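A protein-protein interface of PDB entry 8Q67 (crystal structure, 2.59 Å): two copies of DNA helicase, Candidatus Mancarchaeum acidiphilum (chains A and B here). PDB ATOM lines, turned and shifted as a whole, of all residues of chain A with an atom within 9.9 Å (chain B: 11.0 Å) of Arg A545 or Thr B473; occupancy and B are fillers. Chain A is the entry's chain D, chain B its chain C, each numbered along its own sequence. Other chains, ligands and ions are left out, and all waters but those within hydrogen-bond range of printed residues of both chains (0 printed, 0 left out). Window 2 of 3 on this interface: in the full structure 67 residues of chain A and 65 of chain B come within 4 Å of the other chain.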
ATOM      1  N   LYS A 537      19.820  25.028 -27.969  1.00  0.00           N
ATOM      2  CA  LYS A 537      20.571  23.867 -27.433  1.00  0.00           C
ATOM      3  C   LYS A 537      22.050  24.233 -27.358  1.00  0.00           C
ATOM      4  O   LYS A 537      22.649  24.057 -26.291  1.00  0.00           O
ATOM      5  CB  LYS A 537      20.362  22.653 -28.341  1.00  0.00           C
ATOM      6  CG  LYS A 537      21.069  21.376 -27.915  1.00  0.00           C
ATOM      7  CD  LYS A 537      20.525  20.152 -28.615  1.00  0.00           C
ATOM      8  CE  LYS A 537      21.605  19.161 -28.990  1.00  0.00           C
ATOM      9  NZ  LYS A 537      21.043  17.817 -29.262  1.00  0.00           N
ATOM     10  N   GLU A 538      22.600  24.738 -28.457  1.00  0.00           N
ATOM     11  CA  GLU A 538      24.028  25.117 -28.489  1.00  0.00           C
ATOM     12  C   GLU A 538      24.309  26.071 -27.339  1.00  0.00           C
ATOM     13  O   GLU A 538      25.127  25.724 -26.488  1.00  0.00           O
ATOM     14  CB  GLU A 538      24.327  25.898 -29.765  1.00  0.00           C
ATOM     15  CG  GLU A 538      24.597  25.043 -30.986  1.00  0.00           C
ATOM     16  CD  GLU A 538      24.825  25.877 -32.234  1.00  0.00           C
ATOM     17  OE1 GLU A 538      25.757  26.705 -32.223  1.00  0.00           O
ATOM     18  OE2 GLU A 538      24.064  25.710 -33.205  1.00  0.00           O
ATOM     19  N   TYR A 539      23.651  27.228 -27.334  1.00  0.00           N
ATOM     20  CA  TYR A 539      23.930  28.261 -26.304  1.00  0.00           C
ATOM     21  C   TYR A 539      23.878  27.645 -24.907  1.00  0.00           C
ATOM     22  O   TYR A 539      24.761  27.945 -24.114  1.00  0.00           O
ATOM     23  CB  TYR A 539      22.968  29.439 -26.442  1.00  0.00           C
ATOM     24  CG  TYR A 539      23.131  30.533 -25.421  1.00  0.00           C
ATOM     25  CD1 TYR A 539      24.338  31.188 -25.256  1.00  0.00           C
ATOM     26  CD2 TYR A 539      22.069  30.921 -24.625  1.00  0.00           C
ATOM     27  CE1 TYR A 539      24.488  32.196 -24.320  1.00  0.00           C
ATOM     28  CE2 TYR A 539      22.202  31.927 -23.685  1.00  0.00           C
ATOM     29  CZ  TYR A 539      23.414  32.569 -23.534  1.00  0.00           C
ATOM     30  OH  TYR A 539      23.547  33.558 -22.605  1.00  0.00           O
ATOM     31  N   TYR A 540      22.885  26.804 -24.633  1.00  0.00           N
ATOM     32  CA  TYR A 540      22.828  26.141 -23.310  1.00  0.00           C
ATOM     33  C   TYR A 540      24.103  25.337 -23.086  1.00  0.00           C
ATOM     34  O   TYR A 540      24.830  25.640 -22.138  1.00  0.00           O
ATOM     35  CB  TYR A 540      21.605  25.237 -23.169  1.00  0.00           C
ATOM     36  CG  TYR A 540      21.523  24.517 -21.847  1.00  0.00           C
ATOM     37  CD1 TYR A 540      21.300  25.208 -20.670  1.00  0.00           C
ATOM     38  CD2 TYR A 540      21.683  23.145 -21.772  1.00  0.00           C
ATOM     39  CE1 TYR A 540      21.228  24.555 -19.451  1.00  0.00           C
ATOM     40  CE2 TYR A 540      21.613  22.476 -20.563  1.00  0.00           C
ATOM     41  CZ  TYR A 540      21.384  23.184 -19.399  1.00  0.00           C
ATOM     42  OH  TYR A 540      21.326  22.525 -18.207  1.00  0.00           O
ATOM     43  N   VAL A 541      24.344  24.326 -23.917  1.00  0.00           N
ATOM     44  CA  VAL A 541      25.520  23.445 -23.686  1.00  0.00           C
ATOM     45  C   VAL A 541      26.768  24.323 -23.638  1.00  0.00           C
ATOM     46  O   VAL A 541      27.663  24.036 -22.832  1.00  0.00           O
ATOM     47  CB  VAL A 541      25.614  22.349 -24.758  1.00  0.00           C
ATOM     48  CG1 VAL A 541      26.798  21.429 -24.521  1.00  0.00           C
ATOM     49  CG2 VAL A 541      24.327  21.549 -24.845  1.00  0.00           C
ATOM     50  N   ASP A 542      26.790  25.381 -24.443  1.00  0.00           N
ATOM     51  CA  ASP A 542      27.963  26.221 -24.453  1.00  0.00           C
ATOM     52  C   ASP A 542      28.056  26.990 -23.182  1.00  0.00           C
ATOM     53  O   ASP A 542      29.102  27.159 -22.639  1.00  0.00           O
ATOM     54  CB  ASP A 542      27.915  27.188 -25.611  1.00  0.00           C
ATOM     55  CG  ASP A 542      28.819  26.778 -26.730  1.00  0.00           C
ATOM     56  OD1 ASP A 542      29.571  25.813 -26.545  1.00  0.00           O
ATOM     57  OD2 ASP A 542      28.776  27.412 -27.796  1.00  0.00           O
ATOM     58  N   LEU A 543      26.940  27.488 -22.711  1.00  0.00           N
ATOM     59  CA  LEU A 543      26.910  28.211 -21.472  1.00  0.00           C
ATOM     60  C   LEU A 543      27.289  27.365 -20.281  1.00  0.00           C
ATOM     61  O   LEU A 543      27.829  27.863 -19.321  1.00  0.00           O
ATOM     62  CB  LEU A 543      25.537  28.779 -21.252  1.00  0.00           C
ATOM     63  CG  LEU A 543      25.550  29.873 -20.218  1.00  0.00           C
ATOM     64  CD1 LEU A 543      26.951  30.416 -20.045  1.00  0.00           C
ATOM     65  CD2 LEU A 543      24.605  30.950 -20.689  1.00  0.00           C
ATOM     66  N   ARG A 544      26.898  26.110 -20.289  1.00  0.00           N
ATOM     67  CA  ARG A 544      27.225  25.261 -19.181  1.00  0.00           C
ATOM     68  C   ARG A 544      28.707  25.033 -19.004  1.00  0.00           C
ATOM     69  O   ARG A 544      29.196  25.099 -17.892  1.00  0.00           O
ATOM     70  CB  ARG A 544      26.494  23.937 -19.288  1.00  0.00           C
ATOM     71  CG  ARG A 544      25.005  24.060 -19.061  1.00  0.00           C
ATOM     72  CD  ARG A 544      24.639  23.840 -17.616  1.00  0.00           C
ATOM     73  NE  ARG A 544      24.522  22.427 -17.316  1.00  0.00           N
ATOM     74  CZ  ARG A 544      24.425  21.935 -16.094  1.00  0.00           C
ATOM     75  NH1 ARG A 544      24.422  22.740 -15.051  1.00  0.00           N
ATOM     76  NH2 ARG A 544      24.330  20.633 -15.919  1.00  0.00           N
ATOM     77  N   ARG A 545      29.441  24.775 -20.074  1.00  0.00           N
ATOM     78  CA  ARG A 545      30.857  24.584 -19.869  1.00  0.00           C
ATOM     79  C   ARG A 545      31.318  25.972 -19.560  1.00  0.00           C
ATOM     80  O   ARG A 545      31.008  26.885 -20.293  1.00  0.00           O
ATOM     81  CB  ARG A 545      31.544  24.044 -21.104  1.00  0.00           C
ATOM     82  CG  ARG A 545      30.972  24.558 -22.397  1.00  0.00           C
ATOM     83  CD  ARG A 545      31.906  24.305 -23.563  1.00  0.00           C
ATOM     84  NE  ARG A 545      31.781  22.945 -24.061  1.00  0.00           N
ATOM     85  CZ  ARG A 545      31.155  22.615 -25.182  1.00  0.00           C
ATOM     86  NH1 ARG A 545      30.600  23.550 -25.928  1.00  0.00           N
ATOM     87  NH2 ARG A 545      31.085  21.351 -25.556  1.00  0.00           N
ATOM     88  N   ALA A 546      32.076  26.109 -18.483  1.00  0.00           N
ATOM     89  CA  ALA A 546      32.561  27.397 -17.990  1.00  0.00           C
ATOM     90  C   ALA A 546      31.417  28.370 -17.793  1.00  0.00           C
ATOM     91  O   ALA A 546      30.790  28.372 -16.738  1.00  0.00           O
ATOM     92  CB  ALA A 546      33.656  27.990 -18.873  1.00  0.00           C
ATOM     93  N   ILE A 555      23.279  28.203 -13.852  1.00  0.00           N
ATOM     94  CA  ILE A 555      22.527  28.040 -15.102  1.00  0.00           C
ATOM     95  C   ILE A 555      21.999  26.611 -15.146  1.00  0.00           C
ATOM     96  O   ILE A 555      22.772  25.659 -15.312  1.00  0.00           O
ATOM     97  CB  ILE A 555      23.381  28.343 -16.344  1.00  0.00           C
ATOM     98  CG1 ILE A 555      23.973  29.750 -16.250  1.00  0.00           C
ATOM     99  CG2 ILE A 555      22.578  28.220 -17.648  1.00  0.00           C
ATOM    100  CD1 ILE A 555      22.940  30.851 -16.365  1.00  0.00           C
ATOM    101  N   TYR B 288      13.449  14.192 -17.703  1.00  0.00           N
ATOM    102  CA  TYR B 288      14.474  13.304 -18.230  1.00  0.00           C
ATOM    103  C   TYR B 288      15.280  12.709 -17.082  1.00  0.00           C
ATOM    104  O   TYR B 288      15.591  13.397 -16.107  1.00  0.00           O
ATOM    105  CB  TYR B 288      15.407  14.058 -19.184  1.00  0.00           C
ATOM    106  CG  TYR B 288      16.471  13.184 -19.815  1.00  0.00           C
ATOM    107  CD1 TYR B 288      16.140  12.245 -20.783  1.00  0.00           C
ATOM    108  CD2 TYR B 288      17.805  13.299 -19.443  1.00  0.00           C
ATOM    109  CE1 TYR B 288      17.105  11.440 -21.360  1.00  0.00           C
ATOM    110  CE2 TYR B 288      18.779  12.497 -20.013  1.00  0.00           C
ATOM    111  CZ  TYR B 288      18.423  11.569 -20.968  1.00  0.00           C
ATOM    112  OH  TYR B 288      19.390  10.772 -21.540  1.00  0.00           O
ATOM    113  N   ASP B 469      23.904  18.414  -9.329  1.00  0.00           N
ATOM    114  CA  ASP B 469      24.195  18.872 -10.686  1.00  0.00           C
ATOM    115  C   ASP B 469      25.623  18.457 -11.023  1.00  0.00           C
ATOM    116  O   ASP B 469      26.585  19.109 -10.612  1.00  0.00           O
ATOM    117  CB  ASP B 469      24.003  20.380 -10.774  1.00  0.00           C
ATOM    118  CG  ASP B 469      24.093  20.897 -12.183  1.00  0.00           C
ATOM    119  OD1 ASP B 469      23.052  20.938 -12.868  1.00  0.00           O
ATOM    120  OD2 ASP B 469      25.205  21.271 -12.602  1.00  0.00           O
ATOM    121  N   ILE B 470      25.768  17.358 -11.773  1.00  0.00           N
ATOM    122  CA  ILE B 470      27.094  16.782 -11.997  1.00  0.00           C
ATOM    123  C   ILE B 470      27.896  17.535 -13.041  1.00  0.00           C
ATOM    124  O   ILE B 470      29.052  17.172 -13.293  1.00  0.00           O
ATOM    125  CB  ILE B 470      26.988  15.297 -12.402  1.00  0.00           C
ATOM    126  CG1 ILE B 470      26.461  15.161 -13.830  1.00  0.00           C
ATOM    127  CG2 ILE B 470      26.098  14.550 -11.435  1.00  0.00           C
ATOM    128  CD1 ILE B 470      26.435  13.721 -14.340  1.00  0.00           C
ATOM    129  N   MET B 471      27.326  18.559 -13.619  1.00  0.00           N
ATOM    130  CA  MET B 471      27.973  19.339 -14.631  1.00  0.00           C
ATOM    131  C   MET B 471      28.698  18.583 -15.722  1.00  0.00           C
ATOM    132  O   MET B 471      29.794  18.913 -16.092  1.00  0.00           O
ATOM    133  CB  MET B 471      28.833  20.396 -14.006  1.00  0.00           C
ATOM    134  CG  MET B 471      27.954  21.404 -13.327  1.00  0.00           C
ATOM    135  SD  MET B 471      28.791  22.704 -12.450  1.00  0.00           S
ATOM    136  CE  MET B 471      29.440  23.687 -13.773  1.00  0.00           C
ATOM    137  N   ASP B 472      28.036  17.564 -16.226  1.00  0.00           N
ATOM    138  CA  ASP B 472      28.486  16.774 -17.372  1.00  0.00           C
ATOM    139  C   ASP B 472      27.917  17.355 -18.668  1.00  0.00           C
ATOM    140  O   ASP B 472      26.705  17.577 -18.779  1.00  0.00           O
ATOM    141  CB  ASP B 472      28.063  15.314 -17.219  1.00  0.00           C
ATOM    142  CG  ASP B 472      28.365  14.489 -18.455  1.00  0.00           C
ATOM    143  OD1 ASP B 472      29.314  14.834 -19.197  1.00  0.00           O
ATOM    144  OD2 ASP B 472      27.639  13.500 -18.687  1.00  0.00           O
ATOM    145  N   THR B 473      28.777  17.625 -19.629  1.00  0.00           N
ATOM    146  CA  THR B 473      28.346  18.242 -20.862  1.00  0.00           C
ATOM    147  C   THR B 473      27.455  17.381 -21.720  1.00  0.00           C
ATOM    148  O   THR B 473      26.503  17.874 -22.288  1.00  0.00           O
ATOM    149  CB  THR B 473      29.542  18.750 -21.640  1.00  0.00           C
ATOM    150  OG1 THR B 473      29.890  20.032 -21.127  1.00  0.00           O
ATOM    151  CG2 THR B 473      29.197  18.872 -23.074  1.00  0.00           C
ATOM    152  N   GLU B 474      27.800  16.117 -21.867  1.00  0.00           N
ATOM    153  CA  GLU B 474      26.939  15.197 -22.611  1.00  0.00           C
ATOM    154  C   GLU B 474      25.518  15.243 -22.060  1.00  0.00           C
ATOM    155  O   GLU B 474      24.542  15.352 -22.815  1.00  0.00           O
ATOM    156  CB  GLU B 474      27.448  13.747 -22.529  1.00  0.00           C
ATOM    157  CG  GLU B 474      28.739  13.302 -23.333  1.00  0.00           C
ATOM    158  CD  GLU B 474      28.720  13.542 -24.853  1.00  0.00           C
ATOM    159  OE1 GLU B 474      27.702  13.240 -25.498  1.00  0.00           O
ATOM    160  OE2 GLU B 474      29.710  14.086 -25.400  1.00  0.00           O
ATOM    161  N   LEU B 475      25.397  15.153 -20.724  1.00  0.00           N
ATOM    162  CA  LEU B 475      24.093  15.136 -20.065  1.00  0.00           C
ATOM    163  C   LEU B 475      23.339  16.425 -20.325  1.00  0.00           C
ATOM    164  O   LEU B 475      22.118  16.410 -20.513  1.00  0.00           O
ATOM    165  CB  LEU B 475      24.252  14.930 -18.553  1.00  0.00           C
ATOM    166  CG  LEU B 475      22.976  14.825 -17.702  1.00  0.00           C
ATOM    167  CD1 LEU B 475      22.215  13.546 -18.045  1.00  0.00           C
ATOM    168  CD2 LEU B 475      23.295  14.845 -16.209  1.00  0.00           C
ATOM    169  N   ASP B 476      24.047  17.556 -20.302  1.00  0.00           N
ATOM    170  CA  ASP B 476      23.432  18.816 -20.699  1.00  0.00           C
ATOM    171  C   ASP B 476      22.863  18.716 -22.108  1.00  0.00           C
ATOM    172  O   ASP B 476      21.730  19.146 -22.360  1.00  0.00           O
ATOM    173  CB  ASP B 476      24.453  19.951 -20.624  1.00  0.00           C
ATOM    174  CG  ASP B 476      25.124  20.045 -19.274  1.00  0.00           C
ATOM    175  OD1 ASP B 476      24.701  19.319 -18.349  1.00  0.00           O
ATOM    176  OD2 ASP B 476      26.071  20.846 -19.137  1.00  0.00           O
ATOM    177  N   LYS B 477      23.632  18.142 -23.037  1.00  0.00           N
ATOM    178  CA  LYS B 477      23.148  17.961 -24.404  1.00  0.00           C
ATOM    179  C   LYS B 477      21.845  17.161 -24.417  1.00  0.00           C
ATOM    180  O   LYS B 477      20.863  17.551 -25.066  1.00  0.00           O
ATOM    181  CB  LYS B 477      24.225  17.253 -25.234  1.00  0.00           C
ATOM    182  CG  LYS B 477      25.575  17.985 -25.289  1.00  0.00           C
ATOM    183  CD  LYS B 477      26.695  17.048 -25.713  1.00  0.00           C
ATOM    184  CE  LYS B 477      26.781  16.906 -27.203  1.00  0.00           C
ATOM    185  NZ  LYS B 477      27.263  18.146 -27.899  1.00  0.00           N
ATOM    186  N   SER B 478      21.819  16.036 -23.698  1.00  0.00           N
ATOM    187  CA  SER B 478      20.656  15.145 -23.747  1.00  0.00           C
ATOM    188  C   SER B 478      19.428  15.823 -23.150  1.00  0.00           C
ATOM    189  O   SER B 478      18.315  15.726 -23.688  1.00  0.00           O
ATOM    190  CB  SER B 478      20.967  13.830 -23.023  1.00  0.00           C
ATOM    191  OG  SER B 478      19.885  12.910 -23.087  1.00  0.00           O
ATOM    192  N   ILE B 479      19.621  16.527 -22.038  1.00  0.00           N
ATOM    193  CA  ILE B 479      18.510  17.208 -21.384  1.00  0.00           C
ATOM    194  C   ILE B 479      17.949  18.296 -22.293  1.00  0.00           C
ATOM    195  O   ILE B 479      16.727  18.424 -22.460  1.00  0.00           O
ATOM    196  CB  ILE B 479      18.964  17.747 -20.011  1.00  0.00           C
ATOM    197  CG1 ILE B 479      19.402  16.527 -19.165  1.00  0.00           C
ATOM    198  CG2 ILE B 479      17.923  18.745 -19.423  1.00  0.00           C
ATOM    199  CD1 ILE B 479      19.907  16.927 -17.759  1.00  0.00           C
ATOM    200  N   ALA B 480      18.834  19.074 -22.919  1.00  0.00           N
ATOM    201  CA  ALA B 480      18.369  20.109 -23.836  1.00  0.00           C
ATOM    202  C   ALA B 480      17.593  19.503 -24.996  1.00  0.00           C
ATOM    203  O   ALA B 480      16.585  20.066 -25.438  1.00  0.00           O
ATOM    204  CB  ALA B 480      19.547  20.919 -24.370  1.00  0.00           C
ATOM    205  N   ASN B 481      18.052  18.358 -25.510  1.00  0.00           N
ATOM    206  CA  ASN B 481      17.340  17.736 -26.621  1.00  0.00           C
ATOM    207  C   ASN B 481      15.959  17.250 -26.194  1.00  0.00           C
ATOM    208  O   ASN B 481      14.982  17.444 -26.922  1.00  0.00           O
ATOM    209  CB  ASN B 481      18.153  16.581 -27.205  1.00  0.00           C
ATOM    210  CG  ASN B 481      17.972  16.456 -28.706  1.00  0.00           C
ATOM    211  OD1 ASN B 481      17.986  17.458 -29.419  1.00  0.00           O
ATOM    212  ND2 ASN B 481      17.792  15.231 -29.191  1.00  0.00           N
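The side-chain amide oxygen (OD1) of Asn B481 sits at hydrogen-bond distance from the side-chain amino group (NZ) of Lys A537 (3.1 Å). The side-chain carboxylate (OD2) of Asp B469 is in salt-bridge range of the guanidinium group (NH1) of Arg A544, at 3.0 Å. The side-chain carboxylate (OD1) of Asp B476 is in salt-bridge range of the guanidinium group (NH2) of Arg A544, at 2.8 Å.
The backbone carbonyl oxygen (O) of Ile A555 lies within hydrogen-bond range of the guanidinium group (NH1) of Arg A544 (3.4 Å). The backbone carbonyl oxygen (O) of Asp B472 sits close to the side-chain carboxylate (OD1) of Asp B476 (2.7 Å). The side-chain carboxylate of Asp A542 lies within salt-bridge range of the guanidinium group of Arg A545. NE of Arg A544 lies within hydrogen-bond range of OH of Tyr A540, 3.3 Å away.
Among the printed residues, pairs that only touch across the chains: Val A541 with Lys B477 (3.7 Å), Tyr A540 with Asp B476 (3.8 Å), Val A541 with Thr B473 (3.8 Å), Lys A537 with Ala B480 (3.9 Å) and Arg A545 with Thr B473 (3.98 Å).
Of the printed residues of chain B, Lys A537 touches Ala B480 (3.9 Å) and Asn B481 (3.1 Å). Printed residues of chain B within 4 Å of Tyr A540: Asp B476 (3.8 Å). Printed residues of chain B within 4 Å of Val A541: Thr B473 and Lys B477. No residue of chain B comes within 4 Å of Asp A542. Leu A543 touches none of the printed residues of chain B. Of the printed residues of chain B, Arg A545 touches Thr B473 (3.98 Å). Ala A546 touches none of the printed residues of chain B. Of the printed residues of chain A, Thr B473 touches Val A541 (3.8 Å) and Arg A545 (3.98 Å). Glu B474 touches none of the printed residues of chain A. Of the printed residues of chain A, Ala B480 touches Lys A537. Of the printed residues of chain A, Asn B481 touches Lys A537. The nearest printed residue of chain A that does not touch Thr B473 is Arg A544 (5.5 Å). The nearest printed residue of chain A that does not touch Ala B480 is Tyr A540 (4.03 Å).
Printed residues of chain A that touch a printed residue of chain B: Lys A537, Tyr A540, Val A541, Arg A544 and Arg A545. Hydrophobic or aromatic side chains of chain A within 4 Å of the printed part of chain B: Tyr A540 and Val A541. Hydrophobic or aromatic side chains of chain B within 4 Å of the printed part of chain A: Ala B480.
No position is printed for both chains.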
